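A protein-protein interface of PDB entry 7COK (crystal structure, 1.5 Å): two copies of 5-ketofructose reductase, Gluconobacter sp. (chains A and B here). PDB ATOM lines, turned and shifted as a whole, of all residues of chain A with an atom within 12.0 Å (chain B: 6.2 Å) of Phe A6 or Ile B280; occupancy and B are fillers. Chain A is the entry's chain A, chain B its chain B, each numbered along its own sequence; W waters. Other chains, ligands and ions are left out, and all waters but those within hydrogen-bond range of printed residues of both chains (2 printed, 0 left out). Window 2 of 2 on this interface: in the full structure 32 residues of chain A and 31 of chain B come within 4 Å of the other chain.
No position is printed for both chains.
Of the 10 pairs that touch across the chains among the printed residues, none has its exchanged pair printed and touching as well.
Among the printed residues, merely in contact across the chains: Phe A6 with Asn B21 (3.1 Å), Gly A5 with Ala B19 (3.6 Å), Phe A6 with Ile B280 (3.6 Å), Phe A6 with Pro B22 (3.8 Å), Phe A6 with Val B24 (3.9 Å), Phe A6 with Ala B25 (3.9 Å), Arg A7 with Cys B18 (3.9 Å) and Arg A39 with Val B24 (3.95 Å).
Hydrophobic or aromatic side chains of chain A that line the printed part of chain B: Phe A6.
Along chain A the printed residues that touch a printed residue of chain B span positions 5 to 39.
Printed residues of chain B that touch a printed residue of chain A: Cys B18, Ala B19, Asn B21, Pro B22, Val B24, Ala B25, Asn B42 and Ile B280.
Hydrophobic or aromatic side chains of chain B that line the printed part of chain A: Pro B22, Val B24, Ala B25 and Ile B280.
Printed residues of chain B within 4 Å of Phe A6: Ala B19, Asn B21, Pro B22, Val B24, Ala B25, Asn B42 and Ile B280.
Cys B18 touches one residue of chain A.
Ala B19 touches just these residues of chain A: Gly A5 and Phe A6.
Asn B21 touches one residue of chain A.
Val B24 touches two residues of chain A.
Of chain A, only Phe A6 comes within 4 Å of Ala B25.
Asn B42 touches just one residue of chain A: Phe A6 (3.1 Å).
No residue of chain A comes within 4 Å of Thr B276.
Leu B277 touches none of the printed residues of chain A.
Asn B279 touches none of the printed residues of chain A.
No residue of chain A comes within 4 Å of Phe B281.
Of the printed residues of chain B, Arg A39 touches Val B24.
Of the printed residues of chain B, Gly A5 touches Ala B19 (3.6 Å).
The nearest printed residue of chain B that does not touch Phe A6 is Asp B20 (4.01 Å).
OD1 of Asn B21 is in hydrogen-bond range of OG1 of Thr B23 (2.7 Å).
The backbone carbonyl oxygen of Ile A9 lies within hydrogen-bond range of the backbone NH of Arg A39 (2.8 Å).
The side-chain amide nitrogen of Asn B42 is in hydrogen-bond range of the backbone carbonyl oxygen of Cys B18 (3.0 Å).
NH2 of Arg A7 lies within salt-bridge range of OE1 of Glu A61 (3.0 Å).
Water W2 lies within hydrogen-bond range of the backbone carbonyl oxygen of Asn B42 and the backbone carbonyl oxygen of Ser A8.
Water W1 lies within hydrogen-bond range of the backbone NH of Asn B42 (2.9 Å) and the guanidinium group of Arg A39 (3.0 Å).
The backbone carbonyl oxygen of Ala B19 is in hydrogen-bond range of the backbone NH of Phe A6 (2.8 Å).
The backbone carbonyl oxygen of Phe A6 lies within hydrogen-bond range of the side-chain amide nitrogen of Asn B42, at 3.1 Å.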
ATOM      1  N   GLY A   5       4.073 -20.362   1.379  1.00  0.00           N
ATOM      2  CA  GLY A   5       4.723 -21.218   2.414  1.00  0.00           C
ATOM      3  C   GLY A   5       3.916 -21.260   3.693  1.00  0.00           C
ATOM      4  O   GLY A   5       2.951 -22.009   3.789  1.00  0.00           O
ATOM      5  N   PHE A   6       4.298 -20.423   4.657  1.00  0.00           N
ATOM      6  CA  PHE A   6       3.811 -20.529   6.029  1.00  0.00           C
ATOM      7  C   PHE A   6       2.943 -19.369   6.462  1.00  0.00           C
ATOM      8  O   PHE A   6       2.587 -19.270   7.641  1.00  0.00           O
ATOM      9  CB  PHE A   6       4.991 -20.709   6.971  1.00  0.00           C
ATOM     10  CG  PHE A   6       5.692 -22.008   6.770  1.00  0.00           C
ATOM     11  CD1 PHE A   6       5.116 -23.201   7.208  1.00  0.00           C
ATOM     12  CD2 PHE A   6       6.918 -22.046   6.109  1.00  0.00           C
ATOM     13  CE1 PHE A   6       5.759 -24.421   7.001  1.00  0.00           C
ATOM     14  CE2 PHE A   6       7.564 -23.257   5.901  1.00  0.00           C
ATOM     15  CZ  PHE A   6       6.983 -24.445   6.342  1.00  0.00           C
ATOM     16  N   ARG A   7       2.578 -18.512   5.515  1.00  0.00           N
ATOM     17  CA  ARG A   7       1.652 -17.439   5.813  1.00  0.00           C
ATOM     18  C   ARG A   7       0.240 -17.803   5.393  1.00  0.00           C
ATOM     19  O   ARG A   7      -0.086 -17.746   4.199  1.00  0.00           O
ATOM     20  CB  ARG A   7       2.082 -16.146   5.152  1.00  0.00           C
ATOM     21  CG  ARG A   7       1.153 -15.016   5.518  1.00  0.00           C
ATOM     22  CD  ARG A   7       1.391 -13.811   4.648  1.00  0.00           C
ATOM     23  NE  ARG A   7       0.548 -12.722   5.125  1.00  0.00           N
ATOM     24  CZ  ARG A   7       0.579 -11.468   4.673  1.00  0.00           C
ATOM     25  NH1 ARG A   7       1.425 -11.095   3.721  1.00  0.00           N
ATOM     26  NH2 ARG A   7      -0.230 -10.564   5.217  1.00  0.00           N
ATOM     27  N   SER A   8      -0.575 -18.198   6.376  1.00  0.00           N
ATOM     28  CA  SER A   8      -2.008 -18.451   6.149  1.00  0.00           C
ATOM     29  C   SER A   8      -2.790 -17.150   6.102  1.00  0.00           C
ATOM     30  O   SER A   8      -2.430 -16.188   6.770  1.00  0.00           O
ATOM     31  CB  SER A   8      -2.580 -19.323   7.268  1.00  0.00           C
ATOM     32  OG  SER A   8      -1.810 -20.499   7.475  1.00  0.00           O
ATOM     33  N   ILE A   9      -3.874 -17.133   5.336  1.00  0.00           N
ATOM     34  CA  ILE A   9      -4.828 -16.021   5.325  1.00  0.00           C
ATOM     35  C   ILE A   9      -5.485 -16.028   6.707  1.00  0.00           C
ATOM     36  O   ILE A   9      -5.861 -17.100   7.217  1.00  0.00           O
ATOM     37  CB  ILE A   9      -5.897 -16.200   4.213  1.00  0.00           C
ATOM     38  CG1 ILE A   9      -5.273 -16.183   2.797  1.00  0.00           C
ATOM     39  CG2 ILE A   9      -7.025 -15.178   4.390  1.00  0.00           C
ATOM     40  CD1 ILE A   9      -6.130 -16.761   1.680  1.00  0.00           C
ATOM     41  N   LEU A  10      -5.600 -14.847   7.331  1.00  0.00           N
ATOM     42  CA  LEU A  10      -6.129 -14.761   8.688  1.00  0.00           C
ATOM     43  C   LEU A  10      -7.481 -14.086   8.698  1.00  0.00           C
ATOM     44  O   LEU A  10      -7.675 -13.037   8.080  1.00  0.00           O
ATOM     45  CB  LEU A  10      -5.164 -14.003   9.606  1.00  0.00           C
ATOM     46  CG  LEU A  10      -3.775 -14.664   9.729  1.00  0.00           C
ATOM     47  CD1 LEU A  10      -2.844 -13.761  10.521  1.00  0.00           C
ATOM     48  CD2 LEU A  10      -3.886 -16.062  10.355  1.00  0.00           C
ATOM     49  N   LEU A  36      -8.014 -24.326   1.150  1.00  0.00           N
ATOM     50  CA  LEU A  36      -7.625 -22.930   1.308  1.00  0.00           C
ATOM     51  C   LEU A  36      -6.756 -22.848   2.530  1.00  0.00           C
ATOM     52  O   LEU A  36      -7.116 -23.370   3.606  1.00  0.00           O
ATOM     53  CB  LEU A  36      -8.874 -22.058   1.479  1.00  0.00           C
ATOM     54  CG  LEU A  36      -9.140 -20.815   0.627  1.00  0.00           C
ATOM     55  CD1 LEU A  36     -10.099 -19.893   1.382  1.00  0.00           C
ATOM     56  CD2 LEU A  36      -7.881 -20.073   0.231  1.00  0.00           C
ATOM     57  N   ASP A  37      -5.587 -22.227   2.375  1.00  0.00           N
ATOM     58  CA  ASP A  37      -4.705 -22.017   3.513  1.00  0.00           C
ATOM     59  C   ASP A  37      -5.156 -20.754   4.252  1.00  0.00           C
ATOM     60  O   ASP A  37      -4.599 -19.668   4.097  1.00  0.00           O
ATOM     61  CB  ASP A  37      -3.240 -21.956   3.111  1.00  0.00           C
ATOM     62  CG  ASP A  37      -2.324 -21.704   4.299  1.00  0.00           C
ATOM     63  OD1 ASP A  37      -2.755 -21.960   5.457  1.00  0.00           O
ATOM     64  OD2 ASP A  37      -1.178 -21.242   4.085  1.00  0.00           O
ATOM     65  N   ALA A  38      -6.202 -20.936   5.039  1.00  0.00           N
ATOM     66  CA  ALA A  38      -6.839 -19.842   5.781  1.00  0.00           C
ATOM     67  C   ALA A  38      -7.150 -20.366   7.170  1.00  0.00           C
ATOM     68  O   ALA A  38      -7.343 -21.571   7.366  1.00  0.00           O
ATOM     69  CB  ALA A  38      -8.107 -19.349   5.072  1.00  0.00           C
ATOM     70  N   ARG A  39      -7.176 -19.450   8.144  1.00  0.00           N
ATOM     71  CA  ARG A  39      -7.446 -19.788   9.536  1.00  0.00           C
ATOM     72  C   ARG A  39      -8.488 -18.829  10.074  1.00  0.00           C
ATOM     73  O   ARG A  39      -8.575 -17.700   9.643  1.00  0.00           O
ATOM     74  CB  ARG A  39      -6.167 -19.651  10.348  1.00  0.00           C
ATOM     75  CG  ARG A  39      -5.018 -20.520   9.846  1.00  0.00           C
ATOM     76  CD  ARG A  39      -3.801 -20.392  10.729  1.00  0.00           C
ATOM     77  NE  ARG A  39      -4.009 -21.193  11.929  1.00  0.00           N
ATOM     78  CZ  ARG A  39      -3.091 -21.418  12.856  1.00  0.00           C
ATOM     79  NH1 ARG A  39      -1.877 -20.889  12.752  1.00  0.00           N
ATOM     80  NH2 ARG A  39      -3.410 -22.170  13.889  1.00  0.00           N
ATOM     81  N   ILE A  41      -9.460 -17.300  13.742  1.00  0.00           N
ATOM     82  CA  ILE A  41      -8.949 -17.128  15.087  1.00  0.00           C
ATOM     83  C   ILE A  41     -10.040 -16.593  16.029  1.00  0.00           C
ATOM     84  O   ILE A  41     -10.428 -15.422  15.946  1.00  0.00           O
ATOM     85  CB  ILE A  41      -7.691 -16.202  15.097  1.00  0.00           C
ATOM     86  CG1 ILE A  41      -6.644 -16.619  14.022  1.00  0.00           C
ATOM     87  CG2 ILE A  41      -7.096 -16.120  16.490  1.00  0.00           C
ATOM     88  CD1 ILE A  41      -6.225 -18.075  14.000  1.00  0.00           C
ATOM     89  N   MET A  60      -2.019  -6.872  11.766  1.00  0.00           N
ATOM     90  CA  MET A  60      -1.640  -8.263  11.526  1.00  0.00           C
ATOM     91  C   MET A  60      -2.093  -8.708  10.161  1.00  0.00           C
ATOM     92  O   MET A  60      -1.893  -9.876   9.807  1.00  0.00           O
ATOM     93  CB  MET A  60      -2.229  -9.202  12.573  1.00  0.00           C
ATOM     94  CG  MET A  60      -1.759  -8.996  13.987  1.00  0.00           C
ATOM     95  SD  MET A  60      -2.748  -9.966  15.124  1.00  0.00           S
ATOM     96  CE  MET A  60      -2.234  -9.278  16.694  1.00  0.00           C
ATOM     97  N   GLU A  61      -2.742  -7.805   9.411  1.00  0.00           N
ATOM     98  CA  GLU A  61      -3.125  -8.043   8.008  1.00  0.00           C
ATOM     99  C   GLU A  61      -4.137  -9.191   7.829  1.00  0.00           C
ATOM    100  O   GLU A  61      -4.132  -9.912   6.827  1.00  0.00           O
ATOM    101  CB  GLU A  61      -1.878  -8.190   7.107  1.00  0.00           C
ATOM    102  CG  GLU A  61      -0.977  -6.951   7.256  1.00  0.00           C
ATOM    103  CD  GLU A  61       0.055  -6.734   6.165  1.00  0.00           C
ATOM    104  OE1 GLU A  61       0.153  -7.549   5.225  1.00  0.00           O
ATOM    105  OE2 GLU A  61       0.767  -5.703   6.261  1.00  0.00           O
ATOM    106  N   CYS B  18       7.202 -13.050   6.248  1.00  0.00           N
ATOM    107  CA  CYS B  18       7.033 -14.188   7.159  1.00  0.00           C
ATOM    108  C   CYS B  18       6.719 -15.539   6.495  1.00  0.00           C
ATOM    109  O   CYS B  18       6.677 -16.564   7.186  1.00  0.00           O
ATOM    110  CB  CYS B  18       5.953 -13.873   8.206  1.00  0.00           C
ATOM    111  SG  CYS B  18       4.274 -13.939   7.563  1.00  0.00           S
ATOM    112  N   ALA B  19       6.498 -15.547   5.183  1.00  0.00           N
ATOM    113  CA  ALA B  19       6.074 -16.764   4.468  1.00  0.00           C
ATOM    114  C   ALA B  19       7.095 -17.903   4.511  1.00  0.00           C
ATOM    115  O   ALA B  19       6.706 -19.086   4.455  1.00  0.00           O
ATOM    116  CB  ALA B  19       5.693 -16.442   3.026  1.00  0.00           C
ATOM    117  N   ASP B  20       8.383 -17.565   4.637  1.00  0.00           N
ATOM    118  CA  ASP B  20       9.438 -18.596   4.689  1.00  0.00           C
ATOM    119  C   ASP B  20       9.723 -19.179   6.078  1.00  0.00           C
ATOM    120  O   ASP B  20      10.520 -20.116   6.215  1.00  0.00           O
ATOM    121  CB  ASP B  20      10.740 -18.072   4.058  1.00  0.00           C
ATOM    122  CG  ASP B  20      10.697 -18.050   2.523  1.00  0.00           C
ATOM    123  OD1 ASP B  20       9.698 -18.491   1.904  1.00  0.00           O
ATOM    124  OD2 ASP B  20      11.687 -17.578   1.925  1.00  0.00           O
ATOM    125  N   ASN B  21       9.066 -18.642   7.100  1.00  0.00           N
ATOM    126  CA  ASN B  21       9.337 -19.048   8.468  1.00  0.00           C
ATOM    127  C   ASN B  21       8.509 -20.267   8.899  1.00  0.00           C
ATOM    128  O   ASN B  21       7.293 -20.164   8.973  1.00  0.00           O
ATOM    129  CB  ASN B  21       9.090 -17.866   9.405  1.00  0.00           C
ATOM    130  CG  ASN B  21       9.630 -18.095  10.806  1.00  0.00           C
ATOM    131  OD1 ASN B  21       9.777 -19.241  11.287  1.00  0.00           O
ATOM    132  ND2 ASN B  21       9.919 -16.991  11.489  1.00  0.00           N
ATOM    133  N   PRO B  22       9.158 -21.410   9.185  1.00  0.00           N
ATOM    134  CA  PRO B  22       8.462 -22.646   9.513  1.00  0.00           C
ATOM    135  C   PRO B  22       8.081 -22.830  10.983  1.00  0.00           C
ATOM    136  O   PRO B  22       7.550 -23.890  11.353  1.00  0.00           O
ATOM    137  CB  PRO B  22       9.490 -23.706   9.143  1.00  0.00           C
ATOM    138  CG  PRO B  22      10.795 -23.060   9.465  1.00  0.00           C
ATOM    139  CD  PRO B  22      10.628 -21.614   9.137  1.00  0.00           C
ATOM    140  N   THR B  23       8.397 -21.837  11.826  1.00  0.00           N
ATOM    141  CA  THR B  23       8.173 -21.936  13.261  1.00  0.00           C
ATOM    142  C   THR B  23       6.716 -22.383  13.545  1.00  0.00           C
ATOM    143  O   THR B  23       6.487 -23.267  14.367  1.00  0.00           O
ATOM    144  CB  THR B  23       8.540 -20.619  13.981  1.00  0.00           C
ATOM    145  OG1 THR B  23       9.921 -20.329  13.749  1.00  0.00           O
ATOM    146  CG2 THR B  23       8.335 -20.711  15.504  1.00  0.00           C
ATOM    147  N   VAL B  24       5.748 -21.811  12.832  1.00  0.00           N
ATOM    148  CA  VAL B  24       4.331 -22.171  13.007  1.00  0.00           C
ATOM    149  C   VAL B  24       4.097 -23.694  12.940  1.00  0.00           C
ATOM    150  O   VAL B  24       3.473 -24.271  13.815  1.00  0.00           O
ATOM    151  CB  VAL B  24       3.403 -21.391  12.024  1.00  0.00           C
ATOM    152  CG1 VAL B  24       3.840 -21.545  10.569  1.00  0.00           C
ATOM    153  CG2 VAL B  24       1.937 -21.784  12.218  1.00  0.00           C
ATOM    154  N   ALA B  25       4.638 -24.335  11.917  1.00  0.00           N
ATOM    155  CA  ALA B  25       4.476 -25.779  11.730  1.00  0.00           C
ATOM    156  C   ALA B  25       5.147 -26.595  12.841  1.00  0.00           C
ATOM    157  O   ALA B  25       4.560 -27.527  13.404  1.00  0.00           O
ATOM    158  CB  ALA B  25       5.018 -26.184  10.369  1.00  0.00           C
ATOM    159  N   MET B  26       6.354 -26.174  13.205  1.00  0.00           N
ATOM    160  CA  MET B  26       7.121 -26.825  14.250  1.00  0.00           C
ATOM    161  C   MET B  26       6.434 -26.701  15.612  1.00  0.00           C
ATOM    162  O   MET B  26       6.215 -27.707  16.292  1.00  0.00           O
ATOM    163  CB  MET B  26       8.546 -26.258  14.253  1.00  0.00           C
ATOM    164  CG  MET B  26       9.467 -26.798  15.323  1.00  0.00           C
ATOM    165  SD  MET B  26      10.948 -25.787  15.488  1.00  0.00           S
ATOM    166  CE  MET B  26      10.343 -24.316  16.287  1.00  0.00           C
ATOM    167  N   ASN B  42       1.145 -16.924  12.542  1.00  0.00           N
ATOM    168  CA  ASN B  42       2.258 -16.300  11.816  1.00  0.00           C
ATOM    169  C   ASN B  42       1.779 -15.055  11.034  1.00  0.00           C
ATOM    170  O   ASN B  42       1.139 -15.183  10.000  1.00  0.00           O
ATOM    171  CB  ASN B  42       2.906 -17.348  10.889  1.00  0.00           C
ATOM    172  CG  ASN B  42       4.200 -16.852  10.250  1.00  0.00           C
ATOM    173  OD1 ASN B  42       4.899 -16.038  10.825  1.00  0.00           O
ATOM    174  ND2 ASN B  42       4.525 -17.366   9.060  1.00  0.00           N
ATOM    175  N   GLN B 275      11.515 -33.505  13.757  1.00  0.00           N
ATOM    176  CA  GLN B 275      10.933 -34.267  12.675  1.00  0.00           C
ATOM    177  C   GLN B 275      10.146 -33.362  11.730  1.00  0.00           C
ATOM    178  O   GLN B 275      10.292 -33.463  10.519  1.00  0.00           O
ATOM    179  CB  GLN B 275      10.043 -35.366  13.227  1.00  0.00           C
ATOM    180  CG  GLN B 275      10.221 -36.679  12.493  1.00  0.00           C
ATOM    181  CD  GLN B 275       9.472 -37.808  13.149  1.00  0.00           C
ATOM    182  OE1 GLN B 275       8.247 -37.810  13.174  1.00  0.00           O
ATOM    183  NE2 GLN B 275      10.207 -38.789  13.678  1.00  0.00           N
ATOM    184  N   THR B 276       9.340 -32.462  12.302  1.00  0.00           N
ATOM    185  CA  THR B 276       8.533 -31.536  11.517  1.00  0.00           C
ATOM    186  C   THR B 276       9.411 -30.670  10.615  1.00  0.00           C
ATOM    187  O   THR B 276       9.103 -30.488   9.440  1.00  0.00           O
ATOM    188  CB  THR B 276       7.647 -30.658  12.428  1.00  0.00           C
ATOM    189  OG1 THR B 276       6.881 -31.508  13.285  1.00  0.00           O
ATOM    190  CG2 THR B 276       6.693 -29.763  11.614  1.00  0.00           C
ATOM    191  N   LEU B 277      10.506 -30.141  11.169  1.00  0.00           N
ATOM    192  CA  LEU B 277      11.436 -29.342  10.371  1.00  0.00           C
ATOM    193  C   LEU B 277      12.198 -30.155   9.347  1.00  0.00           C
ATOM    194  O   LEU B 277      12.502 -29.653   8.283  1.00  0.00           O
ATOM    195  CB  LEU B 277      12.445 -28.593  11.244  1.00  0.00           C
ATOM    196  CG  LEU B 277      11.991 -27.465  12.169  1.00  0.00           C
ATOM    197  CD1 LEU B 277      13.243 -26.837  12.762  1.00  0.00           C
ATOM    198  CD2 LEU B 277      11.128 -26.399  11.502  1.00  0.00           C
ATOM    199  N   GLU B 278      12.509 -31.400   9.687  1.00  0.00           N
ATOM    200  CA  GLU B 278      13.189 -32.310   8.763  1.00  0.00           C
ATOM    201  C   GLU B 278      12.347 -32.566   7.525  1.00  0.00           C
ATOM    202  O   GLU B 278      12.874 -32.507   6.412  1.00  0.00           O
ATOM    203  CB  GLU B 278      13.538 -33.616   9.471  1.00  0.00           C
ATOM    204  CG  GLU B 278      14.811 -33.530  10.305  1.00  0.00           C
ATOM    205  CD  GLU B 278      14.924 -34.637  11.344  1.00  0.00           C
ATOM    206  OE1 GLU B 278      14.045 -35.527  11.404  1.00  0.00           O
ATOM    207  OE2 GLU B 278      15.891 -34.613  12.120  1.00  0.00           O
ATOM    208  N   ASN B 279      11.041 -32.806   7.720  1.00  0.00           N
ATOM    209  CA  ASN B 279      10.087 -33.011   6.622  1.00  0.00           C
ATOM    210  C   ASN B 279       9.997 -31.777   5.737  1.00  0.00           C
ATOM    211  O   ASN B 279       9.991 -31.882   4.510  1.00  0.00           O
ATOM    212  CB  ASN B 279       8.671 -33.363   7.126  1.00  0.00           C
ATOM    213  CG  ASN B 279       8.648 -34.454   8.193  1.00  0.00           C
ATOM    214  OD1 ASN B 279       9.486 -35.359   8.216  1.00  0.00           O
ATOM    215  ND2 ASN B 279       7.659 -34.373   9.088  1.00  0.00           N
ATOM    216  N   ILE B 280       9.930 -30.605   6.373  1.00  0.00           N
ATOM    217  CA  ILE B 280       9.761 -29.333   5.657  1.00  0.00           C
ATOM    218  C   ILE B 280      10.928 -29.051   4.720  1.00  0.00           C
ATOM    219  O   ILE B 280      10.716 -28.828   3.521  1.00  0.00           O
ATOM    220  CB  ILE B 280       9.498 -28.155   6.628  1.00  0.00           C
ATOM    221  CG1 ILE B 280       8.091 -28.272   7.224  1.00  0.00           C
ATOM    222  CG2 ILE B 280       9.677 -26.800   5.933  1.00  0.00           C
ATOM    223  CD1 ILE B 280       7.893 -27.489   8.507  1.00  0.00           C
ATOM    224  N   PHE B 281      12.149 -29.087   5.254  1.00  0.00           N
ATOM    225  CA  PHE B 281      13.337 -28.783   4.451  1.00  0.00           C
ATOM    226  C   PHE B 281      13.597 -29.847   3.383  1.00  0.00           C
ATOM    227  O   PHE B 281      14.101 -29.542   2.304  1.00  0.00           O
ATOM    228  CB  PHE B 281      14.575 -28.548   5.333  1.00  0.00           C
ATOM    229  CG  PHE B 281      14.406 -27.450   6.371  1.00  0.00           C
ATOM    230  CD1 PHE B 281      13.753 -26.245   6.070  1.00  0.00           C
ATOM    231  CD2 PHE B 281      14.926 -27.619   7.656  1.00  0.00           C
ATOM    232  CE1 PHE B 281      13.611 -25.250   7.036  1.00  0.00           C
ATOM    233  CE2 PHE B 281      14.790 -26.628   8.626  1.00  0.00           C
ATOM    234  CZ  PHE B 281      14.129 -25.443   8.316  1.00  0.00           C
HETATM  235  O   HOH W   1      -0.528 -18.793  11.000  1.00  0.00           O
HETATM  236  O   HOH W   2      -0.700 -16.790   8.963  1.00  0.00           O
